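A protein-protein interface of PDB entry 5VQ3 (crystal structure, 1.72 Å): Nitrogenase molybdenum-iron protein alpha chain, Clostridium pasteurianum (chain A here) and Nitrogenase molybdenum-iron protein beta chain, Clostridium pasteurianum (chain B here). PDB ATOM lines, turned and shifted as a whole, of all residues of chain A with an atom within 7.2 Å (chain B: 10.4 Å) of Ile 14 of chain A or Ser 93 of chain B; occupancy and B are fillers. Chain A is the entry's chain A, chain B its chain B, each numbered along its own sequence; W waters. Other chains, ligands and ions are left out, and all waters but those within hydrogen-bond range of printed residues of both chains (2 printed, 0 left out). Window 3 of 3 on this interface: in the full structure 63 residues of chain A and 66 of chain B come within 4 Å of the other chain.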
ATOM      1  N   LEU A  10      10.313  17.612  36.556  1.00  0.00           N
ATOM      2  CA  LEU A  10      11.077  18.847  36.416  1.00  0.00           C
ATOM      3  C   LEU A  10      12.564  18.620  36.234  1.00  0.00           C
ATOM      4  O   LEU A  10      13.273  19.493  35.691  1.00  0.00           O
ATOM      5  CB  LEU A  10      10.848  19.752  37.608  1.00  0.00           C
ATOM      6  CG  LEU A  10       9.467  20.377  37.724  1.00  0.00           C
ATOM      7  CD1 LEU A  10       9.416  21.156  39.033  1.00  0.00           C
ATOM      8  CD2 LEU A  10       9.067  21.256  36.533  1.00  0.00           C
ATOM      9  N   GLU A  11      13.042  17.449  36.630  1.00  0.00           N
ATOM     10  CA  GLU A  11      14.488  17.226  36.698  1.00  0.00           C
ATOM     11  C   GLU A  11      15.322  17.616  35.464  1.00  0.00           C
ATOM     12  O   GLU A  11      16.308  18.336  35.599  1.00  0.00           O
ATOM     13  CB  GLU A  11      14.785  15.778  37.078  1.00  0.00           C
ATOM     14  CG  GLU A  11      16.259  15.524  37.374  1.00  0.00           C
ATOM     15  CD  GLU A  11      16.553  14.088  37.795  1.00  0.00           C
ATOM     16  OE1 GLU A  11      17.747  13.733  37.910  1.00  0.00           O
ATOM     17  OE2 GLU A  11      15.603  13.303  38.013  1.00  0.00           O
ATOM     18  N   LYS A  12      14.946  17.147  34.273  1.00  0.00           N
ATOM     19  CA  LYS A  12      15.767  17.304  33.067  1.00  0.00           C
ATOM     20  C   LYS A  12      15.713  18.693  32.426  1.00  0.00           C
ATOM     21  O   LYS A  12      16.533  19.034  31.576  1.00  0.00           O
ATOM     22  CB  LYS A  12      15.312  16.252  32.026  1.00  0.00           C
ATOM     23  CG  LYS A  12      16.362  15.854  31.000  1.00  0.00           C
ATOM     24  CD  LYS A  12      15.883  14.687  30.140  1.00  0.00           C
ATOM     25  CE  LYS A  12      16.871  14.337  29.042  1.00  0.00           C
ATOM     26  NZ  LYS A  12      16.362  13.215  28.195  1.00  0.00           N
ATOM     27  N   TYR A  13      14.736  19.501  32.798  1.00  0.00           N
ATOM     28  CA  TYR A  13      14.619  20.820  32.211  1.00  0.00           C
ATOM     29  C   TYR A  13      15.854  21.672  32.567  1.00  0.00           C
ATOM     30  O   TYR A  13      16.290  21.684  33.727  1.00  0.00           O
ATOM     31  CB  TYR A  13      13.420  21.551  32.735  1.00  0.00           C
ATOM     32  CG  TYR A  13      12.029  21.133  32.295  1.00  0.00           C
ATOM     33  CD1 TYR A  13      11.696  20.978  30.963  1.00  0.00           C
ATOM     34  CD2 TYR A  13      11.011  21.028  33.224  1.00  0.00           C
ATOM     35  CE1 TYR A  13      10.396  20.658  30.591  1.00  0.00           C
ATOM     36  CE2 TYR A  13       9.717  20.699  32.859  1.00  0.00           C
ATOM     37  CZ  TYR A  13       9.408  20.507  31.538  1.00  0.00           C
ATOM     38  OH  TYR A  13       8.089  20.224  31.206  1.00  0.00           O
ATOM     39  N   ILE A  14      16.369  22.429  31.607  1.00  0.00           N
ATOM     40  CA  ILE A  14      17.381  23.455  31.940  1.00  0.00           C
ATOM     41  C   ILE A  14      16.805  24.470  32.923  1.00  0.00           C
ATOM     42  O   ILE A  14      15.579  24.681  33.002  1.00  0.00           O
ATOM     43  CB  ILE A  14      17.910  24.170  30.676  1.00  0.00           C
ATOM     44  CG1 ILE A  14      16.812  25.009  30.017  1.00  0.00           C
ATOM     45  CG2 ILE A  14      18.476  23.136  29.711  1.00  0.00           C
ATOM     46  CD1 ILE A  14      17.211  25.658  28.692  1.00  0.00           C
ATOM     47  N   PRO A  15      17.687  25.159  33.677  1.00  0.00           N
ATOM     48  CA  PRO A  15      17.173  26.015  34.751  1.00  0.00           C
ATOM     49  C   PRO A  15      16.117  27.032  34.379  1.00  0.00           C
ATOM     50  O   PRO A  15      15.156  27.177  35.114  1.00  0.00           O
ATOM     51  CB  PRO A  15      18.435  26.723  35.272  1.00  0.00           C
ATOM     52  CG  PRO A  15      19.544  25.776  34.969  1.00  0.00           C
ATOM     53  CD  PRO A  15      19.157  25.019  33.717  1.00  0.00           C
ATOM     54  N   LYS A  16      16.256  27.748  33.260  1.00  0.00           N
ATOM     55  CA  LYS A  16      15.273  28.784  32.966  1.00  0.00           C
ATOM     56  C   LYS A  16      13.902  28.130  32.680  1.00  0.00           C
ATOM     57  O   LYS A  16      12.853  28.677  32.987  1.00  0.00           O
ATOM     58  CB  LYS A  16      15.716  29.639  31.780  1.00  0.00           C
ATOM     59  CG  LYS A  16      14.751  30.741  31.416  1.00  0.00           C
ATOM     60  CD  LYS A  16      15.163  31.399  30.104  1.00  0.00           C
ATOM     61  CE  LYS A  16      14.265  32.582  29.782  1.00  0.00           C
ATOM     62  NZ  LYS A  16      14.516  33.079  28.403  1.00  0.00           N
ATOM     63  N   THR A  17      13.926  26.996  32.016  1.00  0.00           N
ATOM     64  CA  THR A  17      12.682  26.279  31.679  1.00  0.00           C
ATOM     65  C   THR A  17      12.084  25.623  32.910  1.00  0.00           C
ATOM     66  O   THR A  17      10.866  25.698  33.142  1.00  0.00           O
ATOM     67  CB  THR A  17      12.978  25.243  30.585  1.00  0.00           C
ATOM     68  OG1 THR A  17      13.550  25.938  29.464  1.00  0.00           O
ATOM     69  CG2 THR A  17      11.696  24.525  30.187  1.00  0.00           C
ATOM     70  N   LYS A  18      12.954  25.037  33.723  1.00  0.00           N
ATOM     71  CA  LYS A  18      12.518  24.440  34.997  1.00  0.00           C
ATOM     72  C   LYS A  18      11.729  25.455  35.824  1.00  0.00           C
ATOM     73  O   LYS A  18      10.683  25.153  36.396  1.00  0.00           O
ATOM     74  CB  LYS A  18      13.703  23.887  35.767  1.00  0.00           C
ATOM     75  CG  LYS A  18      13.309  23.026  36.954  1.00  0.00           C
ATOM     76  CD  LYS A  18      14.500  22.335  37.626  1.00  0.00           C
ATOM     77  CE  LYS A  18      14.042  21.817  38.989  1.00  0.00           C
ATOM     78  NZ  LYS A  18      14.978  20.842  39.593  1.00  0.00           N
ATOM     79  N   LYS A  19      12.222  26.680  35.886  1.00  0.00           N
ATOM     80  CA  LYS A  19      11.604  27.684  36.727  1.00  0.00           C
ATOM     81  C   LYS A  19      10.246  28.144  36.205  1.00  0.00           C
ATOM     82  O   LYS A  19       9.336  28.452  36.984  1.00  0.00           O
ATOM     83  CB  LYS A  19      12.554  28.884  36.833  1.00  0.00           C
ATOM     84  CG  LYS A  19      12.418  29.699  38.108  1.00  0.00           C
ATOM     85  CD  LYS A  19      13.765  30.277  38.540  1.00  0.00           C
ATOM     86  CE  LYS A  19      14.364  31.200  37.483  1.00  0.00           C
ATOM     87  NZ  LYS A  19      13.451  32.341  37.186  1.00  0.00           N
ATOM     88  N   THR A  20      10.099  28.227  34.879  1.00  0.00           N
ATOM     89  CA  THR A  20       8.825  28.627  34.314  1.00  0.00           C
ATOM     90  C   THR A  20       7.822  27.447  34.352  1.00  0.00           C
ATOM     91  O   THR A  20       6.621  27.646  34.554  1.00  0.00           O
ATOM     92  CB  THR A  20       8.996  29.186  32.880  1.00  0.00           C
ATOM     93  OG1 THR A  20       7.795  29.848  32.470  1.00  0.00           O
ATOM     94  CG2 THR A  20       9.308  28.122  31.918  1.00  0.00           C
ATOM     95  N   HIS A 447       8.076  15.402  26.841  1.00  0.00           N
ATOM     96  CA  HIS A 447       8.927  15.040  27.992  1.00  0.00           C
ATOM     97  C   HIS A 447       8.075  14.685  29.248  1.00  0.00           C
ATOM     98  O   HIS A 447       8.290  13.640  29.876  1.00  0.00           O
ATOM     99  CB  HIS A 447       9.887  16.180  28.315  1.00  0.00           C
ATOM    100  CG  HIS A 447      10.478  16.070  29.687  1.00  0.00           C
ATOM    101  ND1 HIS A 447      11.501  15.203  29.963  1.00  0.00           N
ATOM    102  CD2 HIS A 447      10.130  16.653  30.865  1.00  0.00           C
ATOM    103  CE1 HIS A 447      11.791  15.271  31.259  1.00  0.00           C
ATOM    104  NE2 HIS A 447      10.962  16.132  31.832  1.00  0.00           N
ATOM    105  N   LEU B  39      15.381  15.551  14.572  1.00  0.00           N
ATOM    106  CA  LEU B  39      14.120  16.154  14.981  1.00  0.00           C
ATOM    107  C   LEU B  39      13.766  17.314  14.050  1.00  0.00           C
ATOM    108  O   LEU B  39      14.448  18.350  14.011  1.00  0.00           O
ATOM    109  CB  LEU B  39      14.180  16.652  16.437  1.00  0.00           C
ATOM    110  CG  LEU B  39      12.869  17.155  17.025  1.00  0.00           C
ATOM    111  CD1 LEU B  39      11.907  16.000  17.129  1.00  0.00           C
ATOM    112  CD2 LEU B  39      13.031  17.757  18.391  1.00  0.00           C
ATOM    113  N   ILE B  84      13.835  30.773  18.171  1.00  0.00           N
ATOM    114  CA  ILE B  84      14.525  29.581  17.719  1.00  0.00           C
ATOM    115  C   ILE B  84      15.726  29.325  18.580  1.00  0.00           C
ATOM    116  O   ILE B  84      16.081  28.197  18.875  1.00  0.00           O
ATOM    117  CB  ILE B  84      14.856  29.597  16.208  1.00  0.00           C
ATOM    118  CG1 ILE B  84      15.285  28.192  15.741  1.00  0.00           C
ATOM    119  CG2 ILE B  84      15.988  30.575  15.896  1.00  0.00           C
ATOM    120  CD1 ILE B  84      15.336  28.006  14.245  1.00  0.00           C
ATOM    121  N   LYS B  85      16.370  30.372  19.058  1.00  0.00           N
ATOM    122  CA  LYS B  85      17.512  30.140  19.952  1.00  0.00           C
ATOM    123  C   LYS B  85      17.087  29.479  21.262  1.00  0.00           C
ATOM    124  O   LYS B  85      17.764  28.594  21.760  1.00  0.00           O
ATOM    125  CB  LYS B  85      18.205  31.458  20.250  1.00  0.00           C
ATOM    126  CG  LYS B  85      18.879  32.028  19.036  1.00  0.00           C
ATOM    127  CD  LYS B  85      19.582  33.319  19.379  1.00  0.00           C
ATOM    128  CE  LYS B  85      19.762  34.165  18.138  1.00  0.00           C
ATOM    129  NZ  LYS B  85      20.583  35.353  18.451  1.00  0.00           N
ATOM    130  N   THR B  86      15.967  29.926  21.813  1.00  0.00           N
ATOM    131  CA  THR B  86      15.395  29.284  22.989  1.00  0.00           C
ATOM    132  C   THR B  86      15.005  27.830  22.679  1.00  0.00           C
ATOM    133  O   THR B  86      15.249  26.953  23.482  1.00  0.00           O
ATOM    134  CB  THR B  86      14.177  30.054  23.495  1.00  0.00           C
ATOM    135  OG1 THR B  86      14.609  31.361  23.908  1.00  0.00           O
ATOM    136  CG2 THR B  86      13.459  29.312  24.646  1.00  0.00           C
ATOM    137  N   ALA B  87      14.405  27.574  21.514  1.00  0.00           N
ATOM    138  CA  ALA B  87      14.011  26.208  21.167  1.00  0.00           C
ATOM    139  C   ALA B  87      15.169  25.254  21.147  1.00  0.00           C
ATOM    140  O   ALA B  87      15.084  24.140  21.668  1.00  0.00           O
ATOM    141  CB  ALA B  87      13.319  26.179  19.819  1.00  0.00           C
ATOM    142  N   VAL B  88      16.258  25.673  20.534  1.00  0.00           N
ATOM    143  CA  VAL B  88      17.428  24.799  20.384  1.00  0.00           C
ATOM    144  C   VAL B  88      17.997  24.385  21.746  1.00  0.00           C
ATOM    145  O   VAL B  88      18.373  23.242  21.950  1.00  0.00           O
ATOM    146  CB  VAL B  88      18.465  25.429  19.441  1.00  0.00           C
ATOM    147  CG1 VAL B  88      19.752  24.630  19.453  1.00  0.00           C
ATOM    148  CG2 VAL B  88      17.896  25.487  18.026  1.00  0.00           C
ATOM    149  N   LYS B  89      18.001  25.310  22.698  1.00  0.00           N
ATOM    150  CA  LYS B  89      18.475  25.004  24.044  1.00  0.00           C
ATOM    151  C   LYS B  89      17.618  23.940  24.703  1.00  0.00           C
ATOM    152  O   LYS B  89      18.121  23.021  25.375  1.00  0.00           O
ATOM    153  CB  LYS B  89      18.474  26.276  24.887  1.00  0.00           C
ATOM    154  CG  LYS B  89      19.516  27.274  24.436  1.00  0.00           C
ATOM    155  CD  LYS B  89      19.399  28.593  25.187  1.00  0.00           C
ATOM    156  CE  LYS B  89      20.189  29.651  24.440  1.00  0.00           C
ATOM    157  NZ  LYS B  89      19.995  31.029  24.961  1.00  0.00           N
ATOM    158  N   ASN B  90      16.310  24.058  24.524  1.00  0.00           N
ATOM    159  CA  ASN B  90      15.395  23.061  25.071  1.00  0.00           C
ATOM    160  C   ASN B  90      15.444  21.747  24.316  1.00  0.00           C
ATOM    161  O   ASN B  90      15.330  20.698  24.926  1.00  0.00           O
ATOM    162  CB  ASN B  90      13.976  23.602  25.144  1.00  0.00           C
ATOM    163  CG  ASN B  90      13.831  24.604  26.253  1.00  0.00           C
ATOM    164  OD1 ASN B  90      14.019  24.258  27.416  1.00  0.00           O
ATOM    165  ND2 ASN B  90      13.490  25.831  25.923  1.00  0.00           N
ATOM    166  N   ILE B  91      15.578  21.808  22.992  1.00  0.00           N
ATOM    167  CA  ILE B  91      15.640  20.580  22.209  1.00  0.00           C
ATOM    168  C   ILE B  91      16.809  19.697  22.567  1.00  0.00           C
ATOM    169  O   ILE B  91      16.665  18.486  22.781  1.00  0.00           O
ATOM    170  CB  ILE B  91      15.649  20.865  20.718  1.00  0.00           C
ATOM    171  CG1 ILE B  91      14.299  21.477  20.320  1.00  0.00           C
ATOM    172  CG2 ILE B  91      15.940  19.608  19.934  1.00  0.00           C
ATOM    173  CD1 ILE B  91      14.351  22.209  18.997  1.00  0.00           C
ATOM    174  N   PHE B  92      17.985  20.270  22.592  1.00  0.00           N
ATOM    175  CA  PHE B  92      19.140  19.440  22.794  1.00  0.00           C
ATOM    176  C   PHE B  92      19.139  18.896  24.209  1.00  0.00           C
ATOM    177  O   PHE B  92      19.480  17.742  24.392  1.00  0.00           O
ATOM    178  CB  PHE B  92      20.423  20.169  22.440  1.00  0.00           C
ATOM    179  CG  PHE B  92      20.711  20.175  20.972  1.00  0.00           C
ATOM    180  CD1 PHE B  92      20.816  18.991  20.272  1.00  0.00           C
ATOM    181  CD2 PHE B  92      20.909  21.354  20.306  1.00  0.00           C
ATOM    182  CE1 PHE B  92      21.065  19.000  18.921  1.00  0.00           C
ATOM    183  CE2 PHE B  92      21.183  21.378  18.964  1.00  0.00           C
ATOM    184  CZ  PHE B  92      21.255  20.190  18.255  1.00  0.00           C
ATOM    185  N   SER B  93      18.649  19.685  25.170  1.00  0.00           N
ATOM    186  CA  SER B  93      18.604  19.269  26.571  1.00  0.00           C
ATOM    187  C   SER B  93      17.553  18.215  26.873  1.00  0.00           C
ATOM    188  O   SER B  93      17.853  17.245  27.572  1.00  0.00           O
ATOM    189  CB  SER B  93      18.452  20.468  27.524  1.00  0.00           C
ATOM    190  OG  SER B  93      17.183  21.121  27.402  1.00  0.00           O
ATOM    191  N   LEU B  94      16.338  18.377  26.353  1.00  0.00           N
ATOM    192  CA  LEU B  94      15.275  17.417  26.661  1.00  0.00           C
ATOM    193  C   LEU B  94      15.269  16.205  25.750  1.00  0.00           C
ATOM    194  O   LEU B  94      14.993  15.121  26.212  1.00  0.00           O
ATOM    195  CB  LEU B  94      13.884  18.041  26.577  1.00  0.00           C
ATOM    196  CG  LEU B  94      13.590  19.057  27.652  1.00  0.00           C
ATOM    197  CD1 LEU B  94      12.285  19.767  27.312  1.00  0.00           C
ATOM    198  CD2 LEU B  94      13.541  18.362  28.992  1.00  0.00           C
ATOM    199  N   TYR B  95      15.563  16.407  24.465  1.00  0.00           N
ATOM    200  CA  TYR B  95      15.241  15.403  23.431  1.00  0.00           C
ATOM    201  C   TYR B  95      16.464  14.910  22.669  1.00  0.00           C
ATOM    202  O   TYR B  95      16.417  13.886  22.032  1.00  0.00           O
ATOM    203  CB  TYR B  95      14.167  15.956  22.506  1.00  0.00           C
ATOM    204  CG  TYR B  95      12.918  16.367  23.255  1.00  0.00           C
ATOM    205  CD1 TYR B  95      12.213  15.450  24.029  1.00  0.00           C
ATOM    206  CD2 TYR B  95      12.422  17.640  23.144  1.00  0.00           C
ATOM    207  CE1 TYR B  95      11.076  15.814  24.695  1.00  0.00           C
ATOM    208  CE2 TYR B  95      11.301  18.017  23.817  1.00  0.00           C
ATOM    209  CZ  TYR B  95      10.631  17.088  24.605  1.00  0.00           C
ATOM    210  OH  TYR B  95       9.481  17.501  25.236  1.00  0.00           O
ATOM    211  N   ASN B  96      17.589  15.621  22.784  1.00  0.00           N
ATOM    212  CA  ASN B  96      18.895  15.125  22.325  1.00  0.00           C
ATOM    213  C   ASN B  96      18.924  14.476  20.919  1.00  0.00           C
ATOM    214  O   ASN B  96      19.441  13.389  20.767  1.00  0.00           O
ATOM    215  CB  ASN B  96      19.452  14.112  23.336  1.00  0.00           C
ATOM    216  CG  ASN B  96      20.934  13.825  23.125  1.00  0.00           C
ATOM    217  OD1 ASN B  96      21.724  14.709  22.806  1.00  0.00           O
ATOM    218  ND2 ASN B  96      21.304  12.575  23.283  1.00  0.00           N
ATOM    219  N   PRO B  97      18.389  15.162  19.883  1.00  0.00           N
ATOM    220  CA  PRO B  97      18.603  14.620  18.552  1.00  0.00           C
ATOM    221  C   PRO B  97      20.076  14.768  18.147  1.00  0.00           C
ATOM    222  O   PRO B  97      20.823  15.506  18.780  1.00  0.00           O
ATOM    223  CB  PRO B  97      17.706  15.504  17.680  1.00  0.00           C
ATOM    224  CG  PRO B  97      17.730  16.832  18.394  1.00  0.00           C
ATOM    225  CD  PRO B  97      17.721  16.475  19.843  1.00  0.00           C
ATOM    226  N   ASP B  98      20.500  14.078  17.108  1.00  0.00           N
ATOM    227  CA  ASP B  98      21.836  14.324  16.555  1.00  0.00           C
ATOM    228  C   ASP B  98      21.817  15.514  15.584  1.00  0.00           C
ATOM    229  O   ASP B  98      22.849  16.147  15.308  1.00  0.00           O
ATOM    230  CB  ASP B  98      22.344  13.050  15.885  1.00  0.00           C
ATOM    231  CG  ASP B  98      22.684  11.950  16.885  1.00  0.00           C
ATOM    232  OD1 ASP B  98      22.720  12.180  18.122  1.00  0.00           O
ATOM    233  OD2 ASP B  98      22.940  10.828  16.412  1.00  0.00           O
ATOM    234  N   ILE B 100      19.034  18.839  14.163  1.00  0.00           N
ATOM    235  CA  ILE B 100      17.757  19.547  14.106  1.00  0.00           C
ATOM    236  C   ILE B 100      17.618  20.030  12.676  1.00  0.00           C
ATOM    237  O   ILE B 100      18.474  20.770  12.200  1.00  0.00           O
ATOM    238  CB  ILE B 100      17.698  20.734  15.093  1.00  0.00           C
ATOM    239  CG1 ILE B 100      17.798  20.228  16.533  1.00  0.00           C
ATOM    240  CG2 ILE B 100      16.436  21.519  14.913  1.00  0.00           C
ATOM    241  CD1 ILE B 100      17.946  21.381  17.510  1.00  0.00           C
ATOM    242  N   GLY B 126      27.533  28.866  21.698  1.00  0.00           N
ATOM    243  CA  GLY B 126      27.716  27.530  22.287  1.00  0.00           C
ATOM    244  C   GLY B 126      26.466  26.707  22.594  1.00  0.00           C
ATOM    245  O   GLY B 126      26.552  25.763  23.358  1.00  0.00           O
ATOM    246  N   SER B 127      25.315  27.045  21.994  1.00  0.00           N
ATOM    247  CA  SER B 127      24.024  26.342  22.243  1.00  0.00           C
ATOM    248  C   SER B 127      23.875  25.054  21.434  1.00  0.00           C
ATOM    249  O   SER B 127      22.987  24.234  21.693  1.00  0.00           O
ATOM    250  CB  SER B 127      22.852  27.250  21.901  1.00  0.00           C
ATOM    251  OG  SER B 127      23.041  28.504  22.505  1.00  0.00           O
ATOM    252  N   ILE B 128      24.735  24.902  20.444  1.00  0.00           N
ATOM    253  CA  ILE B 128      24.818  23.675  19.679  1.00  0.00           C
ATOM    254  C   ILE B 128      25.971  22.860  20.225  1.00  0.00           C
ATOM    255  O   ILE B 128      27.125  23.191  19.988  1.00  0.00           O
ATOM    256  CB  ILE B 128      24.988  23.974  18.172  1.00  0.00           C
ATOM    257  CG1 ILE B 128      23.888  24.942  17.729  1.00  0.00           C
ATOM    258  CG2 ILE B 128      24.958  22.675  17.368  1.00  0.00           C
ATOM    259  CD1 ILE B 128      23.891  25.301  16.253  1.00  0.00           C
ATOM    260  N   PRO B 129      25.666  21.796  20.975  1.00  0.00           N
ATOM    261  CA  PRO B 129      26.717  20.987  21.557  1.00  0.00           C
ATOM    262  C   PRO B 129      27.679  20.418  20.509  1.00  0.00           C
ATOM    263  O   PRO B 129      27.315  20.196  19.363  1.00  0.00           O
ATOM    264  CB  PRO B 129      25.943  19.856  22.240  1.00  0.00           C
ATOM    265  CG  PRO B 129      24.623  20.436  22.561  1.00  0.00           C
ATOM    266  CD  PRO B 129      24.329  21.374  21.432  1.00  0.00           C
ATOM    267  N   LYS B 132      26.828  17.905  17.390  1.00  0.00           N
ATOM    268  CA  LYS B 132      25.425  18.083  16.993  1.00  0.00           C
ATOM    269  C   LYS B 132      25.360  18.997  15.809  1.00  0.00           C
ATOM    270  O   LYS B 132      26.281  19.808  15.566  1.00  0.00           O
ATOM    271  CB  LYS B 132      24.642  18.719  18.133  1.00  0.00           C
ATOM    272  CG  LYS B 132      24.704  17.918  19.420  1.00  0.00           C
ATOM    273  CD  LYS B 132      24.153  16.522  19.237  1.00  0.00           C
ATOM    274  CE  LYS B 132      23.745  15.906  20.550  1.00  0.00           C
ATOM    275  NZ  LYS B 132      23.238  14.524  20.277  1.00  0.00           N
ATOM    276  N   MET B 218      11.956   7.526  20.525  1.00  0.00           N
ATOM    277  CA  MET B 218      11.724   8.815  19.870  1.00  0.00           C
ATOM    278  C   MET B 218      12.322   8.878  18.468  1.00  0.00           C
ATOM    279  O   MET B 218      11.675   9.394  17.530  1.00  0.00           O
ATOM    280  CB  MET B 218      12.287   9.950  20.732  1.00  0.00           C
ATOM    281  CG  MET B 218      12.002  11.286  20.113  1.00  0.00           C
ATOM    282  SD  MET B 218      11.949  12.570  21.357  1.00  0.00           S
ATOM    283  CE  MET B 218      11.873  13.988  20.327  1.00  0.00           C
ATOM    284  N   TYR B 219      13.556   8.390  18.332  1.00  0.00           N
ATOM    285  CA  TYR B 219      14.254   8.327  17.043  1.00  0.00           C
ATOM    286  C   TYR B 219      14.315   6.872  16.594  1.00  0.00           C
ATOM    287  O   TYR B 219      15.101   6.084  17.102  1.00  0.00           O
ATOM    288  CB  TYR B 219      15.677   8.928  17.135  1.00  0.00           C
ATOM    289  CG  TYR B 219      15.627  10.308  17.729  1.00  0.00           C
ATOM    290  CD1 TYR B 219      15.058  11.358  17.049  1.00  0.00           C
ATOM    291  CD2 TYR B 219      16.088  10.544  19.024  1.00  0.00           C
ATOM    292  CE1 TYR B 219      14.950  12.596  17.614  1.00  0.00           C
ATOM    293  CE2 TYR B 219      16.005  11.792  19.593  1.00  0.00           C
ATOM    294  CZ  TYR B 219      15.445  12.816  18.890  1.00  0.00           C
ATOM    295  OH  TYR B 219      15.309  14.055  19.450  1.00  0.00           O
HETATM  296  O   HOH W   1      13.708  28.023  27.938  1.00  0.00           O
HETATM  297  O   HOH W   2      14.819  22.190  29.047  1.00  0.00           O
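Water W1 bridges the side-chain hydroxyl (OG1) of Thr 17 of chain A (2.6 Å) and the side-chain amide nitrogen (ND2) of Asn 90 of chain B (3.0 Å). Water W2 lies within hydrogen-bond range of OD1 of Asn 90 of chain B (2.8 Å), N of Ile 14 of chain A (3.0 Å) and OG of Ser 93 of chain B (3.1 Å).
O of Ser 93 of chain B touches CE of Lys 12 of chain A (3.4 Å). Tyr 13 of chain A touches Leu 94 of chain B. CD1 of Ile 14 of chain A touches OD1 of Asn 90 of chain B, 3.7 Å away. Ile 14 of chain A touches Ser 93 of chain B (CG2 to OG, 3.3 Å). Leu 94 of chain B touches His 447 of chain A (CD2 to ND1, 3.9 Å).
The side-chain amino group (NZ) of Lys 12 of chain A sits at hydrogen-bond distance from the backbone carbonyl oxygen (O) of Leu 94 of chain B. OG1 of Thr 17 of chain A lies within hydrogen-bond range of OD1 of Asn 90 of chain B, 2.7 Å away. The backbone NH of His 447 of chain A is in hydrogen-bond range of the side-chain hydroxyl of Tyr 95 of chain B.
O of Thr 86 of chain B sits at hydrogen-bond distance from ND2 of Asn 90 of chain B. O of Lys 89 of chain B sits at hydrogen-bond distance from OG of Ser 93 of chain B. The side-chain hydroxyl (OG) of Ser 93 of chain B is in hydrogen-bond range of the backbone carbonyl oxygen (O) of Asn 90 of chain B (3.1 Å). The backbone carbonyl oxygen (O) of Tyr 95 of chain B sits at hydrogen-bond distance from the side-chain hydroxyl (OH) of Tyr 219 of chain B (2.8 Å).
Lys 12 of chain A touches just these residues of chain B: Ser 93 and Leu 94. Printed residues of chain B within 4 Å of Tyr 13 of chain A: Leu 94. Of chain B, only Asn 90 and Ser 93 come within 4 Å of Ile 14 of chain A. Thr 17 of chain A touches just one residue of chain B: Asn 90. Printed residues of chain B within 4 Å of His 447 of chain A: Leu 94 and Tyr 95. Printed residues of chain A within 4 Å of Asn 90 of chain B: Ile 14 (3.7 Å) and Thr 17 (2.7 Å). Of chain A, only Lys 12 (3.4 Å) and Ile 14 (3.3 Å) come within 4 Å of Ser 93 of chain B. Of the printed residues of chain A, Leu 94 of chain B touches Lys 12 (3.1 Å), Tyr 13 (3.8 Å) and His 447 (3.9 Å). Printed residues of chain A within 4 Å of Tyr 95 of chain B: His 447. Ser 127 of chain B touches none of the printed residues of chain A.
Of the 12 printed residues of chain A, 5 touch a printed residue of chain B. Printed residues of chain A that touch a printed residue of chain B: Lys 12, Tyr 13, Ile 14, Thr 17 and His 447. Among the printed residues, 8 pairs touch across the chains.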
